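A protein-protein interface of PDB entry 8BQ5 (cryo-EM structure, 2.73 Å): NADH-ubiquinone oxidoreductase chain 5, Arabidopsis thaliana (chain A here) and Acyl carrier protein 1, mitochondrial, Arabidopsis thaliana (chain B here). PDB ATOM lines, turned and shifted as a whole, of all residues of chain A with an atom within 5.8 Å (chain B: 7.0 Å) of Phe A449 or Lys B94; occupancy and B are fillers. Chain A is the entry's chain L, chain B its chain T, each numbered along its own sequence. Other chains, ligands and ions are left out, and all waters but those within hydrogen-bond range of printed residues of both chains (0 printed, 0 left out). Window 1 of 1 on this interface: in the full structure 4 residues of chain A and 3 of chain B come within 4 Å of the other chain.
Glu B91 touches Phe A449. Lys B94 touches Phe A449 (CG to CG, 3.5 Å). Arg A451 touches Ser B121.
Ser A360 touches none of the printed residues of chain B. Of the printed residues of chain B, Glu A362 touches Lys B94 (3.2 Å). Phe A449 touches just these residues of chain B: Glu B91 (3.5 Å) and Lys B94 (3.5 Å). Of the printed residues of chain B, Arg A451 touches Ser B121 (3.8 Å). Printed residues of chain B within 4 Å of Asp A452: Lys B94 (2.7 Å). Of the printed residues of chain A, Glu B91 touches Phe A449. Phe B93 touches none of the printed residues of chain A. Of chain A, only Glu A362, Phe A449 and Asp A452 come within 4 Å of Lys B94. Of the printed residues of chain A, Ser B121 touches Arg A451 (3.8 Å). The nearest printed residue of chain A that does not touch Glu B91 is Gly A450 (4.9 Å).
The side-chain amino group of Lys B94 lies within salt-bridge range of the side-chain carboxylate of Asp A452, 2.7 Å away. OE1 of Glu A362 is in salt-bridge range of NZ of Lys B94, 3.2 Å away.
Of the 12 printed residues of chain B, 3 touch a printed residue of chain A. Printed residues of chain B that touch a printed residue of chain A: Glu B91, Lys B94 and Ser B121. Of the 14 printed residues of chain A, 4 touch a printed residue of chain B. Hydrophobic or aromatic side chains of chain A within 4 Å of the printed part of chain B: Phe A449. Among the printed residues, Asp or Glu carboxylates within 4 Å of a Lys or Arg side-chain nitrogen of the other chain: Glu A362 with Lys B94 and Asp A452 with Lys B94.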
ATOM      1  N   MET A 359      22.989 -20.218 -28.972  1.00  0.00           N
ATOM      2  CA  MET A 359      21.959 -20.711 -28.019  1.00  0.00           C
ATOM      3  C   MET A 359      22.066 -22.230 -27.857  1.00  0.00           C
ATOM      4  O   MET A 359      21.029 -22.860 -27.614  1.00  0.00           O
ATOM      5  CB  MET A 359      20.556 -20.317 -28.491  1.00  0.00           C
ATOM      6  CG  MET A 359      20.298 -18.832 -28.381  1.00  0.00           C
ATOM      7  SD  MET A 359      20.164 -18.339 -26.650  1.00  0.00           S
ATOM      8  CE  MET A 359      18.538 -18.987 -26.268  1.00  0.00           C
ATOM      9  N   SER A 360      23.274 -22.789 -27.967  1.00  0.00           N
ATOM     10  CA  SER A 360      23.504 -24.223 -27.773  1.00  0.00           C
ATOM     11  C   SER A 360      22.531 -25.058 -28.601  1.00  0.00           C
ATOM     12  O   SER A 360      21.801 -25.900 -28.073  1.00  0.00           O
ATOM     13  CB  SER A 360      23.429 -24.606 -26.293  1.00  0.00           C
ATOM     14  OG  SER A 360      24.090 -23.650 -25.481  1.00  0.00           O
ATOM     15  N   GLU A 362      19.744 -24.341 -30.006  1.00  0.00           N
ATOM     16  CA  GLU A 362      18.314 -24.125 -29.849  1.00  0.00           C
ATOM     17  C   GLU A 362      17.764 -23.496 -31.123  1.00  0.00           C
ATOM     18  O   GLU A 362      18.267 -22.468 -31.585  1.00  0.00           O
ATOM     19  CB  GLU A 362      18.040 -23.232 -28.638  1.00  0.00           C
ATOM     20  CG  GLU A 362      16.569 -22.942 -28.374  1.00  0.00           C
ATOM     21  CD  GLU A 362      15.775 -24.191 -28.045  1.00  0.00           C
ATOM     22  OE1 GLU A 362      16.106 -24.865 -27.047  1.00  0.00           O
ATOM     23  OE2 GLU A 362      14.815 -24.497 -28.781  1.00  0.00           O
ATOM     24  N   LYS A 367      11.208 -20.715 -27.455  1.00  0.00           N
ATOM     25  CA  LYS A 367      12.142 -20.821 -26.309  1.00  0.00           C
ATOM     26  C   LYS A 367      13.329 -19.900 -26.578  1.00  0.00           C
ATOM     27  O   LYS A 367      14.472 -20.308 -26.292  1.00  0.00           O
ATOM     28  CB  LYS A 367      12.592 -22.271 -26.099  1.00  0.00           C
ATOM     29  CG  LYS A 367      11.535 -23.185 -25.498  1.00  0.00           C
ATOM     30  CD  LYS A 367      10.968 -22.685 -24.190  1.00  0.00           C
ATOM     31  CE  LYS A 367       9.929 -23.620 -23.612  1.00  0.00           C
ATOM     32  NZ  LYS A 367       8.892 -23.968 -24.613  1.00  0.00           N
ATOM     33  N   MET A 368      13.076 -18.729 -27.159  1.00  0.00           N
ATOM     34  CA  MET A 368      14.160 -17.738 -27.351  1.00  0.00           C
ATOM     35  C   MET A 368      13.720 -16.431 -26.679  1.00  0.00           C
ATOM     36  O   MET A 368      13.498 -16.454 -25.471  1.00  0.00           O
ATOM     37  CB  MET A 368      14.458 -17.518 -28.834  1.00  0.00           C
ATOM     38  CG  MET A 368      15.213 -18.677 -29.449  1.00  0.00           C
ATOM     39  SD  MET A 368      15.469 -18.499 -31.223  1.00  0.00           S
ATOM     40  CE  MET A 368      16.279 -20.054 -31.587  1.00  0.00           C
ATOM     41  N   THR A 446      12.136 -12.369 -22.917  1.00  0.00           N
ATOM     42  CA  THR A 446      12.762 -13.666 -23.136  1.00  0.00           C
ATOM     43  C   THR A 446      11.863 -14.808 -22.678  1.00  0.00           C
ATOM     44  O   THR A 446      11.244 -14.755 -21.612  1.00  0.00           O
ATOM     45  CB  THR A 446      14.114 -13.738 -22.418  1.00  0.00           C
ATOM     46  OG1 THR A 446      14.724 -15.009 -22.672  1.00  0.00           O
ATOM     47  CG2 THR A 446      13.959 -13.537 -20.919  1.00  0.00           C
ATOM     48  N   ASN A 447      11.770 -15.835 -23.519  1.00  0.00           N
ATOM     49  CA  ASN A 447      11.154 -17.102 -23.156  1.00  0.00           C
ATOM     50  C   ASN A 447      12.182 -18.225 -23.141  1.00  0.00           C
ATOM     51  O   ASN A 447      11.819 -19.403 -23.066  1.00  0.00           O
ATOM     52  CB  ASN A 447      10.010 -17.433 -24.111  1.00  0.00           C
ATOM     53  CG  ASN A 447       8.903 -16.399 -24.069  1.00  0.00           C
ATOM     54  OD1 ASN A 447       8.436 -16.016 -22.998  1.00  0.00           O
ATOM     55  ND2 ASN A 447       8.481 -15.937 -25.239  1.00  0.00           N
ATOM     56  N   SER A 448      13.461 -17.872 -23.211  1.00  0.00           N
ATOM     57  CA  SER A 448      14.547 -18.826 -23.321  1.00  0.00           C
ATOM     58  C   SER A 448      14.902 -19.400 -21.951  1.00  0.00           C
ATOM     59  O   SER A 448      14.359 -19.003 -20.917  1.00  0.00           O
ATOM     60  CB  SER A 448      15.757 -18.162 -23.976  1.00  0.00           C
ATOM     61  OG  SER A 448      16.192 -17.054 -23.215  1.00  0.00           O
ATOM     62  N   PHE A 449      15.830 -20.353 -21.949  1.00  0.00           N
ATOM     63  CA  PHE A 449      16.258 -21.031 -20.735  1.00  0.00           C
ATOM     64  C   PHE A 449      17.433 -20.302 -20.098  1.00  0.00           C
ATOM     65  O   PHE A 449      18.221 -19.648 -20.788  1.00  0.00           O
ATOM     66  CB  PHE A 449      16.652 -22.476 -21.036  1.00  0.00           C
ATOM     67  CG  PHE A 449      15.489 -23.381 -21.304  1.00  0.00           C
ATOM     68  CD1 PHE A 449      14.803 -23.972 -20.258  1.00  0.00           C
ATOM     69  CD2 PHE A 449      15.085 -23.648 -22.600  1.00  0.00           C
ATOM     70  CE1 PHE A 449      13.738 -24.811 -20.500  1.00  0.00           C
ATOM     71  CE2 PHE A 449      14.018 -24.486 -22.848  1.00  0.00           C
ATOM     72  CZ  PHE A 449      13.344 -25.069 -21.797  1.00  0.00           C
ATOM     73  N   GLY A 450      17.555 -20.439 -18.777  1.00  0.00           N
ATOM     74  CA  GLY A 450      18.617 -19.749 -18.064  1.00  0.00           C
ATOM     75  C   GLY A 450      20.004 -20.186 -18.489  1.00  0.00           C
ATOM     76  O   GLY A 450      20.900 -19.358 -18.667  1.00  0.00           O
ATOM     77  N   ARG A 451      20.205 -21.496 -18.655  1.00  0.00           N
ATOM     78  CA  ARG A 451      21.525 -21.986 -19.039  1.00  0.00           C
ATOM     79  C   ARG A 451      21.872 -21.597 -20.469  1.00  0.00           C
ATOM     80  O   ARG A 451      23.053 -21.566 -20.836  1.00  0.00           O
ATOM     81  CB  ARG A 451      21.594 -23.502 -18.861  1.00  0.00           C
ATOM     82  CG  ARG A 451      22.937 -24.121 -19.210  1.00  0.00           C
ATOM     83  CD  ARG A 451      22.946 -25.632 -18.988  1.00  0.00           C
ATOM     84  NE  ARG A 451      24.215 -26.276 -19.309  1.00  0.00           N
ATOM     85  CZ  ARG A 451      24.564 -26.693 -20.519  1.00  0.00           C
ATOM     86  NH1 ARG A 451      23.760 -26.545 -21.561  1.00  0.00           N
ATOM     87  NH2 ARG A 451      25.748 -27.271 -20.687  1.00  0.00           N
ATOM     88  N   ASP A 452      20.864 -21.293 -21.286  1.00  0.00           N
ATOM     89  CA  ASP A 452      21.127 -20.883 -22.661  1.00  0.00           C
ATOM     90  C   ASP A 452      21.712 -19.477 -22.721  1.00  0.00           C
ATOM     91  O   ASP A 452      22.686 -19.237 -23.445  1.00  0.00           O
ATOM     92  CB  ASP A 452      19.841 -20.970 -23.482  1.00  0.00           C
ATOM     93  CG  ASP A 452      19.463 -22.399 -23.823  1.00  0.00           C
ATOM     94  OD1 ASP A 452      20.110 -23.329 -23.300  1.00  0.00           O
ATOM     95  OD2 ASP A 452      18.515 -22.592 -24.614  1.00  0.00           O
ATOM     96  N   ILE A 453      21.135 -18.552 -21.952  1.00  0.00           N
ATOM     97  CA  ILE A 453      21.593 -17.128 -22.008  1.00  0.00           C
ATOM     98  C   ILE A 453      22.943 -16.992 -21.292  1.00  0.00           C
ATOM     99  O   ILE A 453      23.673 -16.023 -21.590  1.00  0.00           O
ATOM    100  CB  ILE A 453      20.513 -16.176 -21.449  1.00  0.00           C
ATOM    101  CG1 ILE A 453      19.162 -16.408 -22.124  1.00  0.00           C
ATOM    102  CG2 ILE A 453      20.935 -14.722 -21.576  1.00  0.00           C
ATOM    103  CD1 ILE A 453      19.184 -16.135 -23.605  1.00  0.00           C
ATOM    104  N   SER A 454      23.278 -17.926 -20.401  1.00  0.00           N
ATOM    105  CA  SER A 454      24.550 -17.903 -19.690  1.00  0.00           C
ATOM    106  C   SER A 454      25.726 -18.354 -20.547  1.00  0.00           C
ATOM    107  O   SER A 454      26.874 -18.215 -20.111  1.00  0.00           O
ATOM    108  CB  SER A 454      24.466 -18.779 -18.437  1.00  0.00           C
ATOM    109  OG  SER A 454      23.537 -18.253 -17.508  1.00  0.00           O
ATOM    110  N   ARG B  49      20.608 -25.388  -6.141  1.00  0.00           N
ATOM    111  CA  ARG B  49      19.630 -24.882  -7.143  1.00  0.00           C
ATOM    112  C   ARG B  49      18.304 -25.641  -6.992  1.00  0.00           C
ATOM    113  O   ARG B  49      17.246 -24.989  -7.095  1.00  0.00           O
ATOM    114  CB  ARG B  49      20.197 -24.990  -8.564  1.00  0.00           C
ATOM    115  CG  ARG B  49      21.350 -24.037  -8.842  1.00  0.00           C
ATOM    116  CD  ARG B  49      22.333 -24.605  -9.848  1.00  0.00           C
ATOM    117  NE  ARG B  49      21.700 -24.941 -11.113  1.00  0.00           N
ATOM    118  CZ  ARG B  49      21.861 -24.269 -12.245  1.00  0.00           C
ATOM    119  NH1 ARG B  49      22.649 -23.207 -12.281  1.00  0.00           N
ATOM    120  NH2 ARG B  49      21.233 -24.662 -13.338  1.00  0.00           N
ATOM    121  N   ILE B  89      11.858 -27.713 -12.015  1.00  0.00           N
ATOM    122  CA  ILE B  89      13.199 -28.292 -11.976  1.00  0.00           C
ATOM    123  C   ILE B  89      13.699 -28.558 -13.391  1.00  0.00           C
ATOM    124  O   ILE B  89      14.874 -28.328 -13.705  1.00  0.00           O
ATOM    125  CB  ILE B  89      13.214 -29.570 -11.114  1.00  0.00           C
ATOM    126  CG1 ILE B  89      13.129 -29.211  -9.628  1.00  0.00           C
ATOM    127  CG2 ILE B  89      14.465 -30.389 -11.378  1.00  0.00           C
ATOM    128  CD1 ILE B  89      12.486 -30.284  -8.781  1.00  0.00           C
ATOM    129  N   GLU B  90      12.814 -29.043 -14.267  1.00  0.00           N
ATOM    130  CA  GLU B  90      13.172 -29.220 -15.671  1.00  0.00           C
ATOM    131  C   GLU B  90      13.597 -27.901 -16.297  1.00  0.00           C
ATOM    132  O   GLU B  90      14.613 -27.831 -16.997  1.00  0.00           O
ATOM    133  CB  GLU B  90      11.991 -29.797 -16.450  1.00  0.00           C
ATOM    134  CG  GLU B  90      11.316 -30.980 -15.799  1.00  0.00           C
ATOM    135  CD  GLU B  90      11.693 -32.285 -16.446  1.00  0.00           C
ATOM    136  OE1 GLU B  90      12.837 -32.393 -16.930  1.00  0.00           O
ATOM    137  OE2 GLU B  90      10.845 -33.199 -16.476  1.00  0.00           O
ATOM    138  N   GLU B  91      12.829 -26.841 -16.046  1.00  0.00           N
ATOM    139  CA  GLU B  91      13.095 -25.553 -16.672  1.00  0.00           C
ATOM    140  C   GLU B  91      14.349 -24.894 -16.114  1.00  0.00           C
ATOM    141  O   GLU B  91      14.948 -24.046 -16.786  1.00  0.00           O
ATOM    142  CB  GLU B  91      11.884 -24.641 -16.493  1.00  0.00           C
ATOM    143  CG  GLU B  91      10.866 -24.766 -17.613  1.00  0.00           C
ATOM    144  CD  GLU B  91       9.648 -23.894 -17.398  1.00  0.00           C
ATOM    145  OE1 GLU B  91       9.708 -22.986 -16.545  1.00  0.00           O
ATOM    146  OE2 GLU B  91       8.629 -24.122 -18.083  1.00  0.00           O
ATOM    147  N   GLU B  92      14.757 -25.266 -14.899  1.00  0.00           N
ATOM    148  CA  GLU B  92      15.979 -24.715 -14.325  1.00  0.00           C
ATOM    149  C   GLU B  92      17.226 -25.276 -14.997  1.00  0.00           C
ATOM    150  O   GLU B  92      18.164 -24.524 -15.287  1.00  0.00           O
ATOM    151  CB  GLU B  92      16.019 -24.990 -12.822  1.00  0.00           C
ATOM    152  CG  GLU B  92      17.407 -24.894 -12.220  1.00  0.00           C
ATOM    153  CD  GLU B  92      17.839 -23.461 -11.997  1.00  0.00           C
ATOM    154  OE1 GLU B  92      16.968 -22.566 -12.018  1.00  0.00           O
ATOM    155  OE2 GLU B  92      19.050 -23.226 -11.809  1.00  0.00           O
ATOM    156  N   PHE B  93      17.259 -26.584 -15.248  1.00  0.00           N
ATOM    157  CA  PHE B  93      18.412 -27.235 -15.854  1.00  0.00           C
ATOM    158  C   PHE B  93      18.229 -27.520 -17.340  1.00  0.00           C
ATOM    159  O   PHE B  93      19.161 -28.027 -17.974  1.00  0.00           O
ATOM    160  CB  PHE B  93      18.724 -28.543 -15.117  1.00  0.00           C
ATOM    161  CG  PHE B  93      19.133 -28.354 -13.680  1.00  0.00           C
ATOM    162  CD1 PHE B  93      20.452 -28.096 -13.349  1.00  0.00           C
ATOM    163  CD2 PHE B  93      18.197 -28.440 -12.663  1.00  0.00           C
ATOM    164  CE1 PHE B  93      20.829 -27.926 -12.032  1.00  0.00           C
ATOM    165  CE2 PHE B  93      18.569 -28.268 -11.342  1.00  0.00           C
ATOM    166  CZ  PHE B  93      19.887 -28.010 -11.027  1.00  0.00           C
ATOM    167  N   LYS B  94      17.063 -27.204 -17.910  1.00  0.00           N
ATOM    168  CA  LYS B  94      16.740 -27.485 -19.313  1.00  0.00           C
ATOM    169  C   LYS B  94      16.869 -28.977 -19.624  1.00  0.00           C
ATOM    170  O   LYS B  94      17.603 -29.396 -20.521  1.00  0.00           O
ATOM    171  CB  LYS B  94      17.604 -26.651 -20.264  1.00  0.00           C
ATOM    172  CG  LYS B  94      17.017 -26.469 -21.657  1.00  0.00           C
ATOM    173  CD  LYS B  94      18.063 -25.958 -22.640  1.00  0.00           C
ATOM    174  CE  LYS B  94      17.489 -25.814 -24.043  1.00  0.00           C
ATOM    175  NZ  LYS B  94      18.495 -25.277 -25.004  1.00  0.00           N
ATOM    176  N   LEU B  95      16.126 -29.778 -18.868  1.00  0.00           N
ATOM    177  CA  LEU B  95      16.117 -31.220 -19.045  1.00  0.00           C
ATOM    178  C   LEU B  95      14.735 -31.690 -19.472  1.00  0.00           C
ATOM    179  O   LEU B  95      13.716 -31.063 -19.169  1.00  0.00           O
ATOM    180  CB  LEU B  95      16.532 -31.952 -17.764  1.00  0.00           C
ATOM    181  CG  LEU B  95      17.827 -31.508 -17.094  1.00  0.00           C
ATOM    182  CD1 LEU B  95      17.826 -31.932 -15.635  1.00  0.00           C
ATOM    183  CD2 LEU B  95      19.030 -32.071 -17.830  1.00  0.00           C
ATOM    184  N   GLU B  96      14.716 -32.806 -20.192  1.00  0.00           N
ATOM    185  CA  GLU B  96      13.486 -33.455 -20.633  1.00  0.00           C
ATOM    186  C   GLU B  96      13.443 -34.836 -19.988  1.00  0.00           C
ATOM    187  O   GLU B  96      13.957 -35.809 -20.543  1.00  0.00           O
ATOM    188  CB  GLU B  96      13.414 -33.543 -22.152  1.00  0.00           C
ATOM    189  CG  GLU B  96      12.066 -34.005 -22.673  1.00  0.00           C
ATOM    190  CD  GLU B  96      11.710 -33.383 -24.007  1.00  0.00           C
ATOM    191  OE1 GLU B  96      11.946 -32.170 -24.183  1.00  0.00           O
ATOM    192  OE2 GLU B  96      11.189 -34.109 -24.879  1.00  0.00           O
ATOM    193  N   HIS B 118      22.518 -36.948 -14.377  1.00  0.00           N
ATOM    194  CA  HIS B 118      22.247 -36.668 -15.783  1.00  0.00           C
ATOM    195  C   HIS B 118      23.464 -36.032 -16.441  1.00  0.00           C
ATOM    196  O   HIS B 118      23.951 -35.002 -15.959  1.00  0.00           O
ATOM    197  CB  HIS B 118      21.033 -35.756 -15.916  1.00  0.00           C
ATOM    198  CG  HIS B 118      20.376 -35.823 -17.260  1.00  0.00           C
ATOM    199  ND1 HIS B 118      21.080 -35.707 -18.439  1.00  0.00           N
ATOM    200  CD2 HIS B 118      19.081 -35.997 -17.612  1.00  0.00           C
ATOM    201  CE1 HIS B 118      20.248 -35.806 -19.459  1.00  0.00           C
ATOM    202  NE2 HIS B 118      19.029 -35.982 -18.984  1.00  0.00           N
ATOM    203  N   MET B 120      23.708 -34.276 -19.075  1.00  0.00           N
ATOM    204  CA  MET B 120      23.428 -33.039 -19.790  1.00  0.00           C
ATOM    205  C   MET B 120      22.961 -31.911 -18.879  1.00  0.00           C
ATOM    206  O   MET B 120      22.628 -30.831 -19.376  1.00  0.00           O
ATOM    207  CB  MET B 120      22.392 -33.287 -20.889  1.00  0.00           C
ATOM    208  CG  MET B 120      22.938 -34.000 -22.123  1.00  0.00           C
ATOM    209  SD  MET B 120      23.583 -32.905 -23.410  1.00  0.00           S
ATOM    210  CE  MET B 120      25.222 -32.521 -22.791  1.00  0.00           C
ATOM    211  N   SER B 121      22.933 -32.125 -17.567  1.00  0.00           N
ATOM    212  CA  SER B 121      22.509 -31.074 -16.649  1.00  0.00           C
ATOM    213  C   SER B 121      23.540 -29.951 -16.612  1.00  0.00           C
ATOM    214  O   SER B 121      23.190 -28.771 -16.601  1.00  0.00           O
ATOM    215  CB  SER B 121      22.287 -31.629 -15.242  1.00  0.00           C
ATOM    216  OG  SER B 121      23.487 -31.613 -14.491  1.00  0.00           O
